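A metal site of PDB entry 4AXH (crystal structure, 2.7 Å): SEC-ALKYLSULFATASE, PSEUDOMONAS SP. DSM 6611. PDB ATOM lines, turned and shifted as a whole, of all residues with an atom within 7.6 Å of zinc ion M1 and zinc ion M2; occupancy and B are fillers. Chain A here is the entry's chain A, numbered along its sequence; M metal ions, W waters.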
ATOM      1  N   ASP A 131       8.355  -7.468   4.625  1.00  0.00           N
ATOM      2  CA  ASP A 131       9.374  -6.725   3.851  1.00  0.00           C
ATOM      3  C   ASP A 131      10.500  -7.700   3.448  1.00  0.00           C
ATOM      4  O   ASP A 131      10.698  -8.712   4.140  1.00  0.00           O
ATOM      5  CB  ASP A 131      10.010  -5.686   4.837  1.00  0.00           C
ATOM      6  CG  ASP A 131      10.977  -4.646   4.278  1.00  0.00           C
ATOM      7  OD1 ASP A 131      10.512  -3.547   3.895  1.00  0.00           O
ATOM      8  OD2 ASP A 131      12.192  -4.895   4.322  1.00  0.00           O
ATOM      9  N   PRO A 132      11.360  -7.362   2.434  1.00  0.00           N
ATOM     10  CA  PRO A 132      12.530  -8.196   2.180  1.00  0.00           C
ATOM     11  C   PRO A 132      13.389  -8.493   3.439  1.00  0.00           C
ATOM     12  O   PRO A 132      13.962  -9.567   3.557  1.00  0.00           O
ATOM     13  CB  PRO A 132      13.322  -7.344   1.174  1.00  0.00           C
ATOM     14  CG  PRO A 132      12.298  -6.607   0.428  1.00  0.00           C
ATOM     15  CD  PRO A 132      11.313  -6.236   1.465  1.00  0.00           C
ATOM     16  N   ALA A 133      13.464  -7.554   4.382  1.00  0.00           N
ATOM     17  CA  ALA A 133      14.251  -7.723   5.606  1.00  0.00           C
ATOM     18  C   ALA A 133      13.395  -7.897   6.885  1.00  0.00           C
ATOM     19  O   ALA A 133      12.162  -7.931   6.807  1.00  0.00           O
ATOM     20  CB  ALA A 133      15.236  -6.583   5.756  1.00  0.00           C
ATOM     21  N   ASN A 134      14.047  -8.062   8.035  1.00  0.00           N
ATOM     22  CA  ASN A 134      13.432  -8.226   9.350  1.00  0.00           C
ATOM     23  C   ASN A 134      13.747  -7.035  10.231  1.00  0.00           C
ATOM     24  O   ASN A 134      14.789  -6.367  10.055  1.00  0.00           O
ATOM     25  CB  ASN A 134      13.966  -9.508  10.056  1.00  0.00           C
ATOM     26  CG  ASN A 134      13.851 -10.799   9.281  1.00  0.00           C
ATOM     27  OD1 ASN A 134      13.032 -10.961   8.354  1.00  0.00           O
ATOM     28  ND2 ASN A 134      14.660 -11.755   9.676  1.00  0.00           N
ATOM     29  N   ASP A 148      17.326  -2.311  12.921  1.00  0.00           N
ATOM     30  CA  ASP A 148      16.866  -2.056  11.564  1.00  0.00           C
ATOM     31  C   ASP A 148      15.459  -1.509  11.449  1.00  0.00           C
ATOM     32  O   ASP A 148      14.644  -1.628  12.375  1.00  0.00           O
ATOM     33  CB  ASP A 148      17.224  -3.181  10.574  1.00  0.00           C
ATOM     34  CG  ASP A 148      18.720  -3.345  10.427  1.00  0.00           C
ATOM     35  OD1 ASP A 148      19.451  -2.411  10.781  1.00  0.00           O
ATOM     36  OD2 ASP A 148      19.158  -4.421   9.984  1.00  0.00           O
ATOM     37  N   THR A 151      12.862  -1.772   4.564  1.00  0.00           N
ATOM     38  CA  THR A 151      13.170  -1.112   3.286  1.00  0.00           C
ATOM     39  C   THR A 151      12.389   0.170   3.052  1.00  0.00           C
ATOM     40  O   THR A 151      12.889   1.092   2.406  1.00  0.00           O
ATOM     41  CB  THR A 151      12.863  -2.100   2.112  1.00  0.00           C
ATOM     42  OG1 THR A 151      13.290  -3.405   2.448  1.00  0.00           O
ATOM     43  CG2 THR A 151      13.521  -1.704   0.833  1.00  0.00           C
ATOM     44  N   SER A 178      22.172  -2.065  11.276  1.00  0.00           N
ATOM     45  CA  SER A 178      23.151  -3.151  11.209  1.00  0.00           C
ATOM     46  C   SER A 178      24.247  -2.863  10.152  1.00  0.00           C
ATOM     47  O   SER A 178      25.422  -3.140  10.406  1.00  0.00           O
ATOM     48  CB  SER A 178      22.479  -4.486  10.915  1.00  0.00           C
ATOM     49  OG  SER A 178      21.885  -4.550   9.630  1.00  0.00           O
ATOM     50  N   HIS A 179      23.842  -2.327   8.995  1.00  0.00           N
ATOM     51  CA  HIS A 179      24.737  -2.038   7.876  1.00  0.00           C
ATOM     52  C   HIS A 179      24.114  -1.036   6.872  1.00  0.00           C
ATOM     53  O   HIS A 179      22.909  -0.736   6.957  1.00  0.00           O
ATOM     54  CB  HIS A 179      25.200  -3.348   7.154  1.00  0.00           C
ATOM     55  CG  HIS A 179      24.096  -4.152   6.539  1.00  0.00           C
ATOM     56  ND1 HIS A 179      23.146  -4.793   7.325  1.00  0.00           N
ATOM     57  CD2 HIS A 179      23.858  -4.446   5.245  1.00  0.00           C
ATOM     58  CE1 HIS A 179      22.372  -5.447   6.479  1.00  0.00           C
ATOM     59  NE2 HIS A 179      22.757  -5.265   5.209  1.00  0.00           N
ATOM     60  N   SER A 180      24.947  -0.582   5.920  1.00  0.00           N
ATOM     61  CA  SER A 180      24.589   0.396   4.892  1.00  0.00           C
ATOM     62  C   SER A 180      23.727  -0.112   3.704  1.00  0.00           C
ATOM     63  O   SER A 180      23.969   0.326   2.585  1.00  0.00           O
ATOM     64  CB  SER A 180      25.836   1.141   4.421  1.00  0.00           C
ATOM     65  OG  SER A 180      26.770   0.237   3.872  1.00  0.00           O
ATOM     66  N   HIS A 181      22.701  -0.970   3.943  1.00  0.00           N
ATOM     67  CA  HIS A 181      21.806  -1.407   2.857  1.00  0.00           C
ATOM     68  C   HIS A 181      20.399  -0.863   3.038  1.00  0.00           C
ATOM     69  O   HIS A 181      19.903  -0.795   4.159  1.00  0.00           O
ATOM     70  CB  HIS A 181      21.798  -2.924   2.666  1.00  0.00           C
ATOM     71  CG  HIS A 181      23.042  -3.482   2.056  1.00  0.00           C
ATOM     72  ND1 HIS A 181      23.435  -4.785   2.293  1.00  0.00           N
ATOM     73  CD2 HIS A 181      23.968  -2.892   1.267  1.00  0.00           C
ATOM     74  CE1 HIS A 181      24.586  -4.936   1.635  1.00  0.00           C
ATOM     75  NE2 HIS A 181      24.929  -3.831   0.979  1.00  0.00           N
ATOM     76  N   ILE A 182      19.762  -0.446   1.922  1.00  0.00           N
ATOM     77  CA  ILE A 182      18.431   0.165   1.930  1.00  0.00           C
ATOM     78  C   ILE A 182      17.334  -0.645   2.624  1.00  0.00           C
ATOM     79  O   ILE A 182      16.401  -0.059   3.177  1.00  0.00           O
ATOM     80  CB  ILE A 182      17.987   0.734   0.550  1.00  0.00           C
ATOM     81  CG1 ILE A 182      19.192   1.086  -0.351  1.00  0.00           C
ATOM     82  CG2 ILE A 182      17.080   1.967   0.745  1.00  0.00           C
ATOM     83  CD1 ILE A 182      18.916   1.175  -1.937  1.00  0.00           C
ATOM     84  N   ASP A 183      17.467  -1.966   2.664  1.00  0.00           N
ATOM     85  CA  ASP A 183      16.490  -2.838   3.320  1.00  0.00           C
ATOM     86  C   ASP A 183      16.658  -2.821   4.842  1.00  0.00           C
ATOM     87  O   ASP A 183      15.909  -3.486   5.573  1.00  0.00           O
ATOM     88  CB  ASP A 183      16.512  -4.281   2.746  1.00  0.00           C
ATOM     89  CG  ASP A 183      17.872  -4.943   2.544  1.00  0.00           C
ATOM     90  OD1 ASP A 183      18.855  -4.235   2.186  1.00  0.00           O
ATOM     91  OD2 ASP A 183      17.961  -6.176   2.698  1.00  0.00           O
ATOM     92  N   HIS A 184      17.612  -2.023   5.319  1.00  0.00           N
ATOM     93  CA  HIS A 184      17.900  -1.939   6.736  1.00  0.00           C
ATOM     94  C   HIS A 184      17.699  -0.547   7.336  1.00  0.00           C
ATOM     95  O   HIS A 184      17.324  -0.456   8.514  1.00  0.00           O
ATOM     96  CB  HIS A 184      19.251  -2.595   7.049  1.00  0.00           C
ATOM     97  CG  HIS A 184      19.282  -4.027   6.635  1.00  0.00           C
ATOM     98  ND1 HIS A 184      18.853  -5.029   7.486  1.00  0.00           N
ATOM     99  CD2 HIS A 184      19.597  -4.567   5.442  1.00  0.00           C
ATOM    100  CE1 HIS A 184      18.920  -6.156   6.789  1.00  0.00           C
ATOM    101  NE2 HIS A 184      19.382  -5.934   5.556  1.00  0.00           N
ATOM    102  N   LEU A 249      16.246 -14.948   0.086  1.00  0.00           N
ATOM    103  CA  LEU A 249      16.290 -14.373   1.425  1.00  0.00           C
ATOM    104  C   LEU A 249      15.021 -13.636   1.813  1.00  0.00           C
ATOM    105  O   LEU A 249      14.937 -13.062   2.903  1.00  0.00           O
ATOM    106  CB  LEU A 249      17.512 -13.449   1.589  1.00  0.00           C
ATOM    107  CG  LEU A 249      18.872 -14.070   1.323  1.00  0.00           C
ATOM    108  CD1 LEU A 249      19.933 -12.989   1.335  1.00  0.00           C
ATOM    109  CD2 LEU A 249      19.183 -15.157   2.333  1.00  0.00           C
ATOM    110  N   PHE A 250      14.042 -13.619   0.885  1.00  0.00           N
ATOM    111  CA  PHE A 250      12.712 -12.993   1.008  1.00  0.00           C
ATOM    112  C   PHE A 250      11.855 -13.390  -0.163  1.00  0.00           C
ATOM    113  O   PHE A 250      12.334 -14.111  -1.035  1.00  0.00           O
ATOM    114  CB  PHE A 250      12.790 -11.455   1.107  1.00  0.00           C
ATOM    115  CG  PHE A 250      13.792 -10.807   0.174  1.00  0.00           C
ATOM    116  CD1 PHE A 250      13.447 -10.506  -1.131  1.00  0.00           C
ATOM    117  CD2 PHE A 250      15.094 -10.542   0.605  1.00  0.00           C
ATOM    118  CE1 PHE A 250      14.389  -9.993  -2.007  1.00  0.00           C
ATOM    119  CE2 PHE A 250      16.027 -10.009  -0.267  1.00  0.00           C
ATOM    120  CZ  PHE A 250      15.670  -9.749  -1.579  1.00  0.00           C
ATOM    121  N   GLU A 291      29.578  -8.576   3.785  1.00  0.00           N
ATOM    122  CA  GLU A 291      28.329  -8.470   3.034  1.00  0.00           C
ATOM    123  C   GLU A 291      28.034  -6.982   2.625  1.00  0.00           C
ATOM    124  O   GLU A 291      27.360  -6.748   1.612  1.00  0.00           O
ATOM    125  CB  GLU A 291      27.180  -9.074   3.869  1.00  0.00           C
ATOM    126  CG  GLU A 291      25.857  -9.152   3.131  1.00  0.00           C
ATOM    127  CD  GLU A 291      24.953  -7.967   3.376  1.00  0.00           C
ATOM    128  OE1 GLU A 291      25.254  -7.185   4.315  1.00  0.00           O
ATOM    129  OE2 GLU A 291      23.917  -7.849   2.684  1.00  0.00           O
ATOM    130  N   ALA A 292      28.499  -5.995   3.420  1.00  0.00           N
ATOM    131  CA  ALA A 292      28.321  -4.561   3.172  1.00  0.00           C
ATOM    132  C   ALA A 292      29.571  -3.806   3.585  1.00  0.00           C
ATOM    133  O   ALA A 292      30.247  -4.246   4.518  1.00  0.00           O
ATOM    134  CB  ALA A 292      27.125  -4.024   3.934  1.00  0.00           C
ATOM    135  N   ASP A 295      29.329  -2.273   8.048  1.00  0.00           N
ATOM    136  CA  ASP A 295      28.634  -3.474   8.551  1.00  0.00           C
ATOM    137  C   ASP A 295      29.069  -3.870   9.951  1.00  0.00           C
ATOM    138  O   ASP A 295      30.190  -3.607  10.357  1.00  0.00           O
ATOM    139  CB  ASP A 295      28.970  -4.618   7.558  1.00  0.00           C
ATOM    140  CG  ASP A 295      28.225  -5.923   7.648  1.00  0.00           C
ATOM    141  OD1 ASP A 295      27.087  -5.918   8.173  1.00  0.00           O
ATOM    142  OD2 ASP A 295      28.757  -6.931   7.158  1.00  0.00           O
ATOM    143  N   ALA A 309      23.268  -9.647  11.394  1.00  0.00           N
ATOM    144  CA  ALA A 309      22.814  -8.802  10.292  1.00  0.00           C
ATOM    145  C   ALA A 309      22.546  -9.732   9.072  1.00  0.00           C
ATOM    146  O   ALA A 309      21.774 -10.689   9.225  1.00  0.00           O
ATOM    147  CB  ALA A 309      23.870  -7.749   9.974  1.00  0.00           C
ATOM    148  N   ASP A 310      23.219  -9.483   7.914  1.00  0.00           N
ATOM    149  CA  ASP A 310      23.158 -10.280   6.672  1.00  0.00           C
ATOM    150  C   ASP A 310      24.472 -11.039   6.412  1.00  0.00           C
ATOM    151  O   ASP A 310      24.715 -11.512   5.274  1.00  0.00           O
ATOM    152  CB  ASP A 310      22.886  -9.396   5.452  1.00  0.00           C
ATOM    153  CG  ASP A 310      21.630  -8.573   5.488  1.00  0.00           C
ATOM    154  OD1 ASP A 310      20.898  -8.659   6.506  1.00  0.00           O
ATOM    155  OD2 ASP A 310      21.371  -7.852   4.504  1.00  0.00           O
ATOM    156  N   ASN A 311      25.335 -11.130   7.466  1.00  0.00           N
ATOM    157  CA  ASN A 311      26.633 -11.759   7.386  1.00  0.00           C
ATOM    158  C   ASN A 311      26.623 -13.272   7.274  1.00  0.00           C
ATOM    159  O   ASN A 311      27.610 -13.852   6.795  1.00  0.00           O
ATOM    160  CB  ASN A 311      27.500 -11.303   8.537  1.00  0.00           C
ATOM    161  CG  ASN A 311      27.705  -9.835   8.498  1.00  0.00           C
ATOM    162  OD1 ASN A 311      28.043  -9.273   7.449  1.00  0.00           O
ATOM    163  ND2 ASN A 311      27.395  -9.180   9.599  1.00  0.00           N
ATOM    164  N   HIS A 317      25.185 -16.312   0.109  1.00  0.00           N
ATOM    165  CA  HIS A 317      24.982 -14.903  -0.286  1.00  0.00           C
ATOM    166  C   HIS A 317      25.803 -14.618  -1.551  1.00  0.00           C
ATOM    167  O   HIS A 317      26.497 -15.523  -2.065  1.00  0.00           O
ATOM    168  CB  HIS A 317      25.336 -13.948   0.859  1.00  0.00           C
ATOM    169  CG  HIS A 317      24.512 -12.691   0.955  1.00  0.00           C
ATOM    170  ND1 HIS A 317      24.172 -11.952  -0.180  1.00  0.00           N
ATOM    171  CD2 HIS A 317      24.045 -12.048   2.058  1.00  0.00           C
ATOM    172  CE1 HIS A 317      23.503 -10.896   0.260  1.00  0.00           C
ATOM    173  NE2 HIS A 317      23.397 -10.902   1.600  1.00  0.00           N
ATOM    174  N   ARG A 328      32.931  -8.716  -3.626  1.00  0.00           N
ATOM    175  CA  ARG A 328      33.136  -8.768  -2.182  1.00  0.00           C
ATOM    176  C   ARG A 328      34.300  -9.692  -1.852  1.00  0.00           C
ATOM    177  O   ARG A 328      34.738 -10.470  -2.711  1.00  0.00           O
ATOM    178  CB  ARG A 328      31.840  -9.223  -1.475  1.00  0.00           C
ATOM    179  CG  ARG A 328      30.804  -8.175  -1.515  1.00  0.00           C
ATOM    180  CD  ARG A 328      29.453  -8.784  -1.482  1.00  0.00           C
ATOM    181  NE  ARG A 328      28.411  -7.773  -1.251  1.00  0.00           N
ATOM    182  CZ  ARG A 328      27.103  -8.010  -1.355  1.00  0.00           C
ATOM    183  NH1 ARG A 328      26.670  -9.239  -1.681  1.00  0.00           N
ATOM    184  NH2 ARG A 328      26.221  -7.033  -1.150  1.00  0.00           N
ATOM    185  N   GLN A 354      18.757 -10.535  10.103  1.00  0.00           N
ATOM    186  CA  GLN A 354      17.935  -9.485   9.525  1.00  0.00           C
ATOM    187  C   GLN A 354      17.274  -9.918   8.206  1.00  0.00           C
ATOM    188  O   GLN A 354      16.618  -9.142   7.500  1.00  0.00           O
ATOM    189  CB  GLN A 354      18.694  -8.151   9.472  1.00  0.00           C
ATOM    190  CG  GLN A 354      19.205  -7.696  10.851  1.00  0.00           C
ATOM    191  CD  GLN A 354      18.062  -7.388  11.795  1.00  0.00           C
ATOM    192  OE1 GLN A 354      17.637  -8.202  12.622  1.00  0.00           O
ATOM    193  NE2 GLN A 354      17.533  -6.198  11.708  1.00  0.00           N
ATOM    194  N   HIS A 355      17.417 -11.194   7.890  1.00  0.00           N
ATOM    195  CA  HIS A 355      16.754 -11.899   6.819  1.00  0.00           C
ATOM    196  C   HIS A 355      16.559 -13.258   7.382  1.00  0.00           C
ATOM    197  O   HIS A 355      17.479 -13.777   8.014  1.00  0.00           O
ATOM    198  CB  HIS A 355      17.603 -11.982   5.551  1.00  0.00           C
ATOM    199  CG  HIS A 355      17.682 -10.693   4.819  1.00  0.00           C
ATOM    200  ND1 HIS A 355      16.592 -10.149   4.208  1.00  0.00           N
ATOM    201  CD2 HIS A 355      18.739  -9.876   4.642  1.00  0.00           C
ATOM    202  CE1 HIS A 355      17.008  -9.030   3.667  1.00  0.00           C
ATOM    203  NE2 HIS A 355      18.307  -8.826   3.901  1.00  0.00           N
ATOM    204  N   TYR A 417      20.300 -17.637  -3.118  1.00  0.00           N
ATOM    205  CA  TYR A 417      20.466 -16.213  -3.371  1.00  0.00           C
ATOM    206  C   TYR A 417      21.717 -16.063  -4.171  1.00  0.00           C
ATOM    207  O   TYR A 417      21.642 -15.789  -5.368  1.00  0.00           O
ATOM    208  CB  TYR A 417      20.562 -15.446  -2.039  1.00  0.00           C
ATOM    209  CG  TYR A 417      20.250 -13.977  -2.174  1.00  0.00           C
ATOM    210  CD1 TYR A 417      18.947 -13.543  -2.360  1.00  0.00           C
ATOM    211  CD2 TYR A 417      21.252 -13.004  -2.063  1.00  0.00           C
ATOM    212  CE1 TYR A 417      18.640 -12.185  -2.475  1.00  0.00           C
ATOM    213  CE2 TYR A 417      20.964 -11.657  -2.176  1.00  0.00           C
ATOM    214  CZ  TYR A 417      19.659 -11.242  -2.401  1.00  0.00           C
ATOM    215  OH  TYR A 417      19.346  -9.909  -2.538  1.00  0.00           O
HETATM  216 ZN    ZN M   1      22.555  -6.349   3.441  1.00  0.00          ZN
HETATM  217 ZN    ZN M   2      19.408  -7.181   3.959  1.00  0.00          ZN
HETATM  218  O   HOH W   1      20.665  -6.249   2.553  1.00  0.00           O
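The side-chain hydroxyl of Ser 178 sits at hydrogen-bond distance from a ring nitrogen (ND1) of His 179 (2.6 Å). A ring nitrogen (ND1) of His 355 is in hydrogen-bond range of the backbone carbonyl oxygen (O) of Pro 132 (2.8 Å). The side-chain carboxylate (OD2) of Asp 148 is in hydrogen-bond range of a ring nitrogen (ND1) of His 184 (2.6 Å). A ring nitrogen (NE2) of His 317 lies close to the side-chain carboxylate of Glu 291 (3.3 Å). O of Glu 291 lies within hydrogen-bond range of NH2 of Arg 328 (3.0 Å). The backbone NH (N) of His 355 sits close to the side-chain amide nitrogen (ND2) of Asn 134.
Within 4 Å of zinc ion M1: His 179, His 181, His 184, Glu 291 and Asp 310. The nearest printed residue that does not touch zinc ion M1 is Asp 183 (4.4 Å).
Along chain A the residues within 4 Å of zinc ion M2 span positions 183 to 355. The nearest printed residue that does not touch zinc ion M2 is His 179 (4.1 Å).
Zinc ion M1 is bound by a ring nitrogen (NE2) of His 179 (2.1 Å), water W1 (2.1 Å), a ring nitrogen (ND1) of His 181 (2.1 Å), the side-chain carboxylate of Glu 291 (2.2 Å) and the side-chain carboxylate of Asp 310 (2.2 Å). Zinc ion M1 has five donor atoms within binding distance.
Zinc ion M2 is bound by a ring nitrogen (NE2) of His 355 (2.0 Å), a ring nitrogen (NE2) of His 184 (2.0 Å), water W1 (2.1 Å), the side-chain carboxylate of Asp 310 (2.1 Å) and the side-chain carboxylate of Asp 183 (2.2 Å). Zinc ion M2 has five donor atoms within binding distance.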
